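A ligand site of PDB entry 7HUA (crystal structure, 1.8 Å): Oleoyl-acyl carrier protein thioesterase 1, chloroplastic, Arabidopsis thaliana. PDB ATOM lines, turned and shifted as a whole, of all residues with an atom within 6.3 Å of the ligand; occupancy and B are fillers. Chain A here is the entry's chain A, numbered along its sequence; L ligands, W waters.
The guanidinium group (NH1) of Arg 103 sits at hydrogen-bond distance from a nitrogen (N2) of the ligand (3.1 Å). N3 of the ligand sits close to SG of Cys 93.
NH2 of Arg 103 sits at hydrogen-bond distance from ND1 of His 44, at 3.0 Å. N of Ser 121 lies within hydrogen-bond range of O of Arg 103 (2.9 Å). O of Cys 93 lies close to SG of Cys 148 (3.3 Å). O of Arg 102 sits close to SG of Cys 93 (3.8 Å). N of Trp 123 is in hydrogen-bond range of O of Thr 101, at 3.0 Å. The backbone NH (N) of Phe 50 lies within hydrogen-bond range of the backbone carbonyl oxygen (O) of Ala 45 (3.1 Å). The backbone carbonyl oxygen of Phe 50 is in hydrogen-bond range of the side-chain amide nitrogen of Gln 46, 3.2 Å away. The side-chain sulfur (SG) of Cys 148 lies within hydrogen-bond range of the backbone carbonyl oxygen (O) of Tyr 144 (3.6 Å).
His 44 touches the ligand. CA of Ala 45 touches C6 of the ligand, at 3.7 Å. CG2 of Val 48 touches C6 of the ligand, 3.7 Å away. Phe 50 touches the ligand (CE2 to O1, 3.6 Å). Phe 55 touches the ligand. Ala 56 touches the ligand (CB to N1, 3.7 Å). CD1 of Trp 68 touches C3 of the ligand, 3.5 Å away. Thr 101 touches the ligand. Trp 123 touches the ligand. CB of Tyr 144 touches O1 of the ligand (3.9 Å). Phe 147 touches the ligand. Hydrophobic or aromatic side chains that line the ligand: His 44, Val 48, Phe 50, Phe 55, Ala 56, Trp 68, Trp 123, Tyr 144 and Phe 147. 13 residues have an atom within 4 Å of the ligand: His 44, Ala 45, Val 48, Phe 50, Phe 55, Ala 56, Trp 68, Cys 93, Thr 101, Arg 103, Trp 123, Tyr 144 and Phe 147.
Water W1 lies within hydrogen-bond range of O of Ala 56 (2.8 Å), NE1 of Trp 68 (2.8 Å) and N1 of the ligand (2.9 Å).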
ATOM      1  N   LEU A   9     -30.953  27.522 -17.686  1.00  0.00           N
ATOM      2  CA  LEU A   9     -31.548  26.544 -16.754  1.00  0.00           C
ATOM      3  C   LEU A   9     -31.263  25.061 -17.090  1.00  0.00           C
ATOM      4  O   LEU A   9     -31.788  24.153 -16.434  1.00  0.00           O
ATOM      5  CB  LEU A   9     -33.057  26.797 -16.653  1.00  0.00           C
ATOM      6  CG  LEU A   9     -33.505  28.128 -16.010  1.00  0.00           C
ATOM      7  CD1 LEU A   9     -35.022  28.139 -15.897  1.00  0.00           C
ATOM      8  CD2 LEU A   9     -32.903  28.301 -14.633  1.00  0.00           C
ATOM      9  N   GLY A  41     -22.633  16.888 -15.427  1.00  0.00           N
ATOM     10  CA  GLY A  41     -23.146  17.373 -14.153  1.00  0.00           C
ATOM     11  C   GLY A  41     -22.139  18.245 -13.417  1.00  0.00           C
ATOM     12  O   GLY A  41     -22.509  19.259 -12.837  1.00  0.00           O
ATOM     13  N   HIS A  44     -21.829  21.523 -15.371  1.00  0.00           N
ATOM     14  CA  HIS A  44     -22.998  22.343 -15.118  1.00  0.00           C
ATOM     15  C   HIS A  44     -22.846  23.123 -13.782  1.00  0.00           C
ATOM     16  O   HIS A  44     -22.953  24.344 -13.784  1.00  0.00           O
ATOM     17  CB  HIS A  44     -24.290  21.512 -15.181  1.00  0.00           C
ATOM     18  CG  HIS A  44     -25.550  22.283 -14.937  1.00  0.00           C
ATOM     19  ND1 HIS A  44     -26.715  21.652 -14.538  1.00  0.00           N
ATOM     20  CD2 HIS A  44     -25.803  23.611 -15.106  1.00  0.00           C
ATOM     21  CE1 HIS A  44     -27.627  22.594 -14.444  1.00  0.00           C
ATOM     22  NE2 HIS A  44     -27.125  23.807 -14.751  1.00  0.00           N
ATOM     23  N   ALA A  45     -22.461  22.460 -12.691  1.00  0.00           N
ATOM     24  CA  ALA A  45     -22.266  23.106 -11.380  1.00  0.00           C
ATOM     25  C   ALA A  45     -21.138  24.162 -11.405  1.00  0.00           C
ATOM     26  O   ALA A  45     -21.302  25.254 -10.827  1.00  0.00           O
ATOM     27  CB  ALA A  45     -21.991  22.034 -10.315  1.00  0.00           C
ATOM     28  N   GLN A  46     -20.038  23.881 -12.121  1.00  0.00           N
ATOM     29  CA  GLN A  46     -18.924  24.812 -12.227  1.00  0.00           C
ATOM     30  C   GLN A  46     -19.298  26.070 -13.016  1.00  0.00           C
ATOM     31  O   GLN A  46     -18.776  27.133 -12.726  1.00  0.00           O
ATOM     32  CB  GLN A  46     -17.715  24.155 -12.916  1.00  0.00           C
ATOM     33  CG  GLN A  46     -16.949  23.112 -12.076  1.00  0.00           C
ATOM     34  CD  GLN A  46     -16.597  23.563 -10.673  1.00  0.00           C
ATOM     35  OE1 GLN A  46     -15.801  24.491 -10.476  1.00  0.00           O
ATOM     36  NE2 GLN A  46     -17.185  22.914  -9.681  1.00  0.00           N
ATOM     37  N   VAL A  48     -22.170  27.640 -13.040  1.00  0.00           N
ATOM     38  CA  VAL A  48     -23.017  28.552 -12.235  1.00  0.00           C
ATOM     39  C   VAL A  48     -22.359  28.942 -10.875  1.00  0.00           C
ATOM     40  O   VAL A  48     -23.068  29.400  -9.965  1.00  0.00           O
ATOM     41  CB  VAL A  48     -24.475  28.058 -12.050  1.00  0.00           C
ATOM     42  CG1 VAL A  48     -25.194  27.977 -13.395  1.00  0.00           C
ATOM     43  CG2 VAL A  48     -24.504  26.709 -11.351  1.00  0.00           C
ATOM     44  N   PHE A  50     -20.367  27.059  -8.538  1.00  0.00           N
ATOM     45  CA  PHE A  50     -20.087  26.125  -7.431  1.00  0.00           C
ATOM     46  C   PHE A  50     -18.607  25.693  -7.331  1.00  0.00           C
ATOM     47  O   PHE A  50     -17.880  25.733  -8.336  1.00  0.00           O
ATOM     48  CB  PHE A  50     -21.004  24.890  -7.484  1.00  0.00           C
ATOM     49  CG  PHE A  50     -22.434  25.156  -7.091  1.00  0.00           C
ATOM     50  CD1 PHE A  50     -22.794  25.287  -5.759  1.00  0.00           C
ATOM     51  CD2 PHE A  50     -23.427  25.283  -8.053  1.00  0.00           C
ATOM     52  CE1 PHE A  50     -24.123  25.514  -5.399  1.00  0.00           C
ATOM     53  CE2 PHE A  50     -24.755  25.510  -7.693  1.00  0.00           C
ATOM     54  CZ  PHE A  50     -25.097  25.609  -6.359  1.00  0.00           C
ATOM     55  N   PHE A  55     -20.631  17.909  -4.044  1.00  0.00           N
ATOM     56  CA  PHE A  55     -21.350  18.314  -5.260  1.00  0.00           C
ATOM     57  C   PHE A  55     -22.334  19.424  -4.972  1.00  0.00           C
ATOM     58  O   PHE A  55     -23.300  19.213  -4.215  1.00  0.00           O
ATOM     59  CB  PHE A  55     -22.030  17.144  -6.005  1.00  0.00           C
ATOM     60  CG  PHE A  55     -22.650  17.584  -7.320  1.00  0.00           C
ATOM     61  CD1 PHE A  55     -21.884  17.649  -8.481  1.00  0.00           C
ATOM     62  CD2 PHE A  55     -23.991  17.899  -7.409  1.00  0.00           C
ATOM     63  CE1 PHE A  55     -22.453  18.036  -9.681  1.00  0.00           C
ATOM     64  CE2 PHE A  55     -24.549  18.316  -8.619  1.00  0.00           C
ATOM     65  CZ  PHE A  55     -23.787  18.359  -9.750  1.00  0.00           C
ATOM     66  N   ALA A  56     -22.105  20.604  -5.579  1.00  0.00           N
ATOM     67  CA  ALA A  56     -22.975  21.765  -5.519  1.00  0.00           C
ATOM     68  C   ALA A  56     -23.294  22.259  -4.092  1.00  0.00           C
ATOM     69  O   ALA A  56     -24.443  22.570  -3.788  1.00  0.00           O
ATOM     70  CB  ALA A  56     -24.277  21.514  -6.310  1.00  0.00           C
ATOM     71  N   THR A  58     -23.869  24.778  -1.324  1.00  0.00           N
ATOM     72  CA  THR A  58     -24.236  26.197  -1.273  1.00  0.00           C
ATOM     73  C   THR A  58     -23.516  26.884  -0.113  1.00  0.00           C
ATOM     74  O   THR A  58     -22.964  26.215   0.772  1.00  0.00           O
ATOM     75  CB  THR A  58     -25.770  26.370  -1.161  1.00  0.00           C
ATOM     76  OG1 THR A  58     -26.221  26.208   0.202  1.00  0.00           O
ATOM     77  CG2 THR A  58     -26.553  25.477  -2.123  1.00  0.00           C
ATOM     78  N   TRP A  68     -24.621  17.326  -0.380  1.00  0.00           N
ATOM     79  CA  TRP A  68     -25.579  16.562  -1.163  1.00  0.00           C
ATOM     80  C   TRP A  68     -24.971  15.178  -1.397  1.00  0.00           C
ATOM     81  O   TRP A  68     -23.799  15.103  -1.801  1.00  0.00           O
ATOM     82  CB  TRP A  68     -25.786  17.203  -2.560  1.00  0.00           C
ATOM     83  CG  TRP A  68     -26.671  18.410  -2.564  1.00  0.00           C
ATOM     84  CD1 TRP A  68     -26.303  19.687  -2.848  1.00  0.00           C
ATOM     85  CD2 TRP A  68     -28.060  18.455  -2.245  1.00  0.00           C
ATOM     86  NE1 TRP A  68     -27.384  20.508  -2.788  1.00  0.00           N
ATOM     87  CE2 TRP A  68     -28.475  19.790  -2.397  1.00  0.00           C
ATOM     88  CE3 TRP A  68     -29.015  17.493  -1.917  1.00  0.00           C
ATOM     89  CZ2 TRP A  68     -29.796  20.187  -2.202  1.00  0.00           C
ATOM     90  CZ3 TRP A  68     -30.302  17.891  -1.648  1.00  0.00           C
ATOM     91  CH2 TRP A  68     -30.694  19.226  -1.828  1.00  0.00           C
ATOM     92  N   TRP A  92     -30.152  18.950 -16.225  1.00  0.00           N
ATOM     93  CA  TRP A  92     -30.745  19.995 -15.420  1.00  0.00           C
ATOM     94  C   TRP A  92     -31.049  19.461 -14.009  1.00  0.00           C
ATOM     95  O   TRP A  92     -31.132  18.259 -13.813  1.00  0.00           O
ATOM     96  CB  TRP A  92     -32.028  20.569 -16.056  1.00  0.00           C
ATOM     97  CG  TRP A  92     -33.182  19.595 -16.173  1.00  0.00           C
ATOM     98  CD1 TRP A  92     -34.223  19.447 -15.305  1.00  0.00           C
ATOM     99  CD2 TRP A  92     -33.405  18.646 -17.242  1.00  0.00           C
ATOM    100  NE1 TRP A  92     -35.103  18.494 -15.772  1.00  0.00           N
ATOM    101  CE2 TRP A  92     -34.605  17.955 -16.942  1.00  0.00           C
ATOM    102  CE3 TRP A  92     -32.718  18.317 -18.406  1.00  0.00           C
ATOM    103  CZ2 TRP A  92     -35.132  16.965 -17.789  1.00  0.00           C
ATOM    104  CZ3 TRP A  92     -33.201  17.300 -19.206  1.00  0.00           C
ATOM    105  CH2 TRP A  92     -34.423  16.672 -18.925  1.00  0.00           C
ATOM    106  N   CYS A  93     -31.272  20.376 -13.053  1.00  0.00           N
ATOM    107  CA  CYS A  93     -31.626  19.972 -11.709  1.00  0.00           C
ATOM    108  C   CYS A  93     -32.995  20.506 -11.371  1.00  0.00           C
ATOM    109  O   CYS A  93     -33.347  21.599 -11.795  1.00  0.00           O
ATOM    110  CB  CYS A  93     -30.584  20.461 -10.704  1.00  0.00           C
ATOM    111  SG  CYS A  93     -30.947  19.985  -8.988  1.00  0.00           S
ATOM    112  N   THR A 101     -33.414  17.101  -4.060  1.00  0.00           N
ATOM    113  CA  THR A 101     -33.306  17.516  -5.456  1.00  0.00           C
ATOM    114  C   THR A 101     -33.235  16.295  -6.406  1.00  0.00           C
ATOM    115  O   THR A 101     -33.091  15.164  -5.967  1.00  0.00           O
ATOM    116  CB  THR A 101     -32.098  18.432  -5.663  1.00  0.00           C
ATOM    117  OG1 THR A 101     -30.919  17.778  -5.171  1.00  0.00           O
ATOM    118  CG2 THR A 101     -32.278  19.773  -5.005  1.00  0.00           C
ATOM    119  N   ARG A 102     -33.336  16.535  -7.714  1.00  0.00           N
ATOM    120  CA  ARG A 102     -33.316  15.474  -8.708  1.00  0.00           C
ATOM    121  C   ARG A 102     -32.568  15.988  -9.927  1.00  0.00           C
ATOM    122  O   ARG A 102     -32.877  17.088 -10.383  1.00  0.00           O
ATOM    123  CB  ARG A 102     -34.764  15.185  -9.104  1.00  0.00           C
ATOM    124  CG  ARG A 102     -34.933  13.867  -9.846  1.00  0.00           C
ATOM    125  CD  ARG A 102     -36.274  13.765 -10.538  1.00  0.00           C
ATOM    126  NE  ARG A 102     -36.354  14.660 -11.698  1.00  0.00           N
ATOM    127  CZ  ARG A 102     -37.187  15.695 -11.786  1.00  0.00           C
ATOM    128  NH1 ARG A 102     -37.178  16.464 -12.859  1.00  0.00           N
ATOM    129  NH2 ARG A 102     -38.027  15.971 -10.802  1.00  0.00           N
ATOM    130  N   ARG A 103     -31.573  15.232 -10.426  1.00  0.00           N
ATOM    131  CA  ARG A 103     -30.871  15.619 -11.623  1.00  0.00           C
ATOM    132  C   ARG A 103     -31.215  14.635 -12.732  1.00  0.00           C
ATOM    133  O   ARG A 103     -31.150  13.418 -12.561  1.00  0.00           O
ATOM    134  CB  ARG A 103     -29.342  15.738 -11.392  1.00  0.00           C
ATOM    135  CG  ARG A 103     -28.534  15.948 -12.699  1.00  0.00           C
ATOM    136  CD  ARG A 103     -27.081  16.314 -12.412  1.00  0.00           C
ATOM    137  NE  ARG A 103     -26.993  17.626 -11.762  1.00  0.00           N
ATOM    138  CZ  ARG A 103     -26.961  18.781 -12.428  1.00  0.00           C
ATOM    139  NH1 ARG A 103     -26.914  19.935 -11.760  1.00  0.00           N
ATOM    140  NH2 ARG A 103     -26.963  18.801 -13.755  1.00  0.00           N
ATOM    141  N   SER A 121     -31.560  10.942 -11.183  1.00  0.00           N
ATOM    142  CA  SER A 121     -30.877  10.680  -9.922  1.00  0.00           C
ATOM    143  C   SER A 121     -31.539  11.451  -8.777  1.00  0.00           C
ATOM    144  O   SER A 121     -31.920  12.603  -8.966  1.00  0.00           O
ATOM    145  CB  SER A 121     -29.417  11.069 -10.033  1.00  0.00           C
ATOM    146  OG  SER A 121     -29.344  12.435 -10.420  1.00  0.00           O
ATOM    147  N   TRP A 123     -31.200  13.019  -4.953  1.00  0.00           N
ATOM    148  CA  TRP A 123     -30.164  13.537  -4.080  1.00  0.00           C
ATOM    149  C   TRP A 123     -30.765  13.987  -2.742  1.00  0.00           C
ATOM    150  O   TRP A 123     -31.831  14.597  -2.706  1.00  0.00           O
ATOM    151  CB  TRP A 123     -29.468  14.739  -4.749  1.00  0.00           C
ATOM    152  CG  TRP A 123     -28.678  14.382  -5.978  1.00  0.00           C
ATOM    153  CD1 TRP A 123     -29.151  14.157  -7.230  1.00  0.00           C
ATOM    154  CD2 TRP A 123     -27.255  14.270  -6.062  1.00  0.00           C
ATOM    155  NE1 TRP A 123     -28.112  13.922  -8.092  1.00  0.00           N
ATOM    156  CE2 TRP A 123     -26.934  13.962  -7.399  1.00  0.00           C
ATOM    157  CE3 TRP A 123     -26.219  14.351  -5.124  1.00  0.00           C
ATOM    158  CZ2 TRP A 123     -25.622  13.771  -7.824  1.00  0.00           C
ATOM    159  CZ3 TRP A 123     -24.907  14.191  -5.557  1.00  0.00           C
ATOM    160  CH2 TRP A 123     -24.621  13.936  -6.889  1.00  0.00           C
ATOM    161  N   TYR A 144     -30.240  27.614  -4.387  1.00  0.00           N
ATOM    162  CA  TYR A 144     -30.033  26.828  -5.609  1.00  0.00           C
ATOM    163  C   TYR A 144     -31.238  26.827  -6.573  1.00  0.00           C
ATOM    164  O   TYR A 144     -31.049  26.566  -7.773  1.00  0.00           O
ATOM    165  CB  TYR A 144     -29.552  25.377  -5.341  1.00  0.00           C
ATOM    166  CG  TYR A 144     -30.544  24.496  -4.607  1.00  0.00           C
ATOM    167  CD1 TYR A 144     -31.630  23.939  -5.250  1.00  0.00           C
ATOM    168  CD2 TYR A 144     -30.331  24.151  -3.279  1.00  0.00           C
ATOM    169  CE1 TYR A 144     -32.563  23.175  -4.564  1.00  0.00           C
ATOM    170  CE2 TYR A 144     -31.226  23.353  -2.597  1.00  0.00           C
ATOM    171  CZ  TYR A 144     -32.355  22.871  -3.230  1.00  0.00           C
ATOM    172  OH  TYR A 144     -33.236  22.052  -2.565  1.00  0.00           O
ATOM    173  N   PHE A 147     -31.124  28.295 -10.249  1.00  0.00           N
ATOM    174  CA  PHE A 147     -30.476  27.627 -11.402  1.00  0.00           C
ATOM    175  C   PHE A 147     -31.319  26.453 -11.953  1.00  0.00           C
ATOM    176  O   PHE A 147     -30.880  25.743 -12.849  1.00  0.00           O
ATOM    177  CB  PHE A 147     -29.082  27.105 -11.002  1.00  0.00           C
ATOM    178  CG  PHE A 147     -28.205  28.114 -10.288  1.00  0.00           C
ATOM    179  CD1 PHE A 147     -27.805  29.277 -10.915  1.00  0.00           C
ATOM    180  CD2 PHE A 147     -27.862  27.936  -8.961  1.00  0.00           C
ATOM    181  CE1 PHE A 147     -27.015  30.208 -10.256  1.00  0.00           C
ATOM    182  CE2 PHE A 147     -27.082  28.868  -8.299  1.00  0.00           C
ATOM    183  CZ  PHE A 147     -26.668  30.000  -8.944  1.00  0.00           C
ATOM    184  N   CYS A 148     -32.538  26.274 -11.422  1.00  0.00           N
ATOM    185  CA  CYS A 148     -33.411  25.141 -11.741  1.00  0.00           C
ATOM    186  C   CYS A 148     -34.635  25.622 -12.466  1.00  0.00           C
ATOM    187  O   CYS A 148     -35.222  26.630 -12.043  1.00  0.00           O
ATOM    188  CB  CYS A 148     -33.840  24.435 -10.445  1.00  0.00           C
ATOM    189  SG  CYS A 148     -32.494  23.772  -9.438  1.00  0.00           S
HETATM  190  N1  LIG L   1     -27.811  22.164  -7.093  1.00  0.00           N
HETATM  191  C1  LIG L   1     -27.821  21.135  -7.886  1.00  0.00           C
HETATM  192  C2  LIG L   1     -28.149  19.761  -7.404  1.00  0.00           C
HETATM  193  C3  LIG L   1     -27.319  19.265  -6.209  1.00  0.00           C
HETATM  194  C4  LIG L   1     -27.624  17.797  -6.213  1.00  0.00           C
HETATM  195  C5  LIG L   1     -27.900  17.462  -7.680  1.00  0.00           C
HETATM  196  N2  LIG L   1     -27.689  21.441  -9.205  1.00  0.00           N
HETATM  197  C6  LIG L   1     -25.924  23.348 -10.992  1.00  0.00           C
HETATM  198  O1  LIG L   1     -27.587  23.250  -7.969  1.00  0.00           O
HETATM  199  C7  LIG L   1     -27.276  23.631 -10.348  1.00  0.00           C
HETATM  200  C8  LIG L   1     -28.403  23.463 -11.351  1.00  0.00           C
HETATM  201  C9  LIG L   1     -27.491  22.718  -9.187  1.00  0.00           C
HETATM  202  N3  LIG L   1     -27.843  18.749  -8.404  1.00  0.00           N
HETATM  203  O   HOH W   1     -27.193  22.888  -4.340  1.00  0.00           O
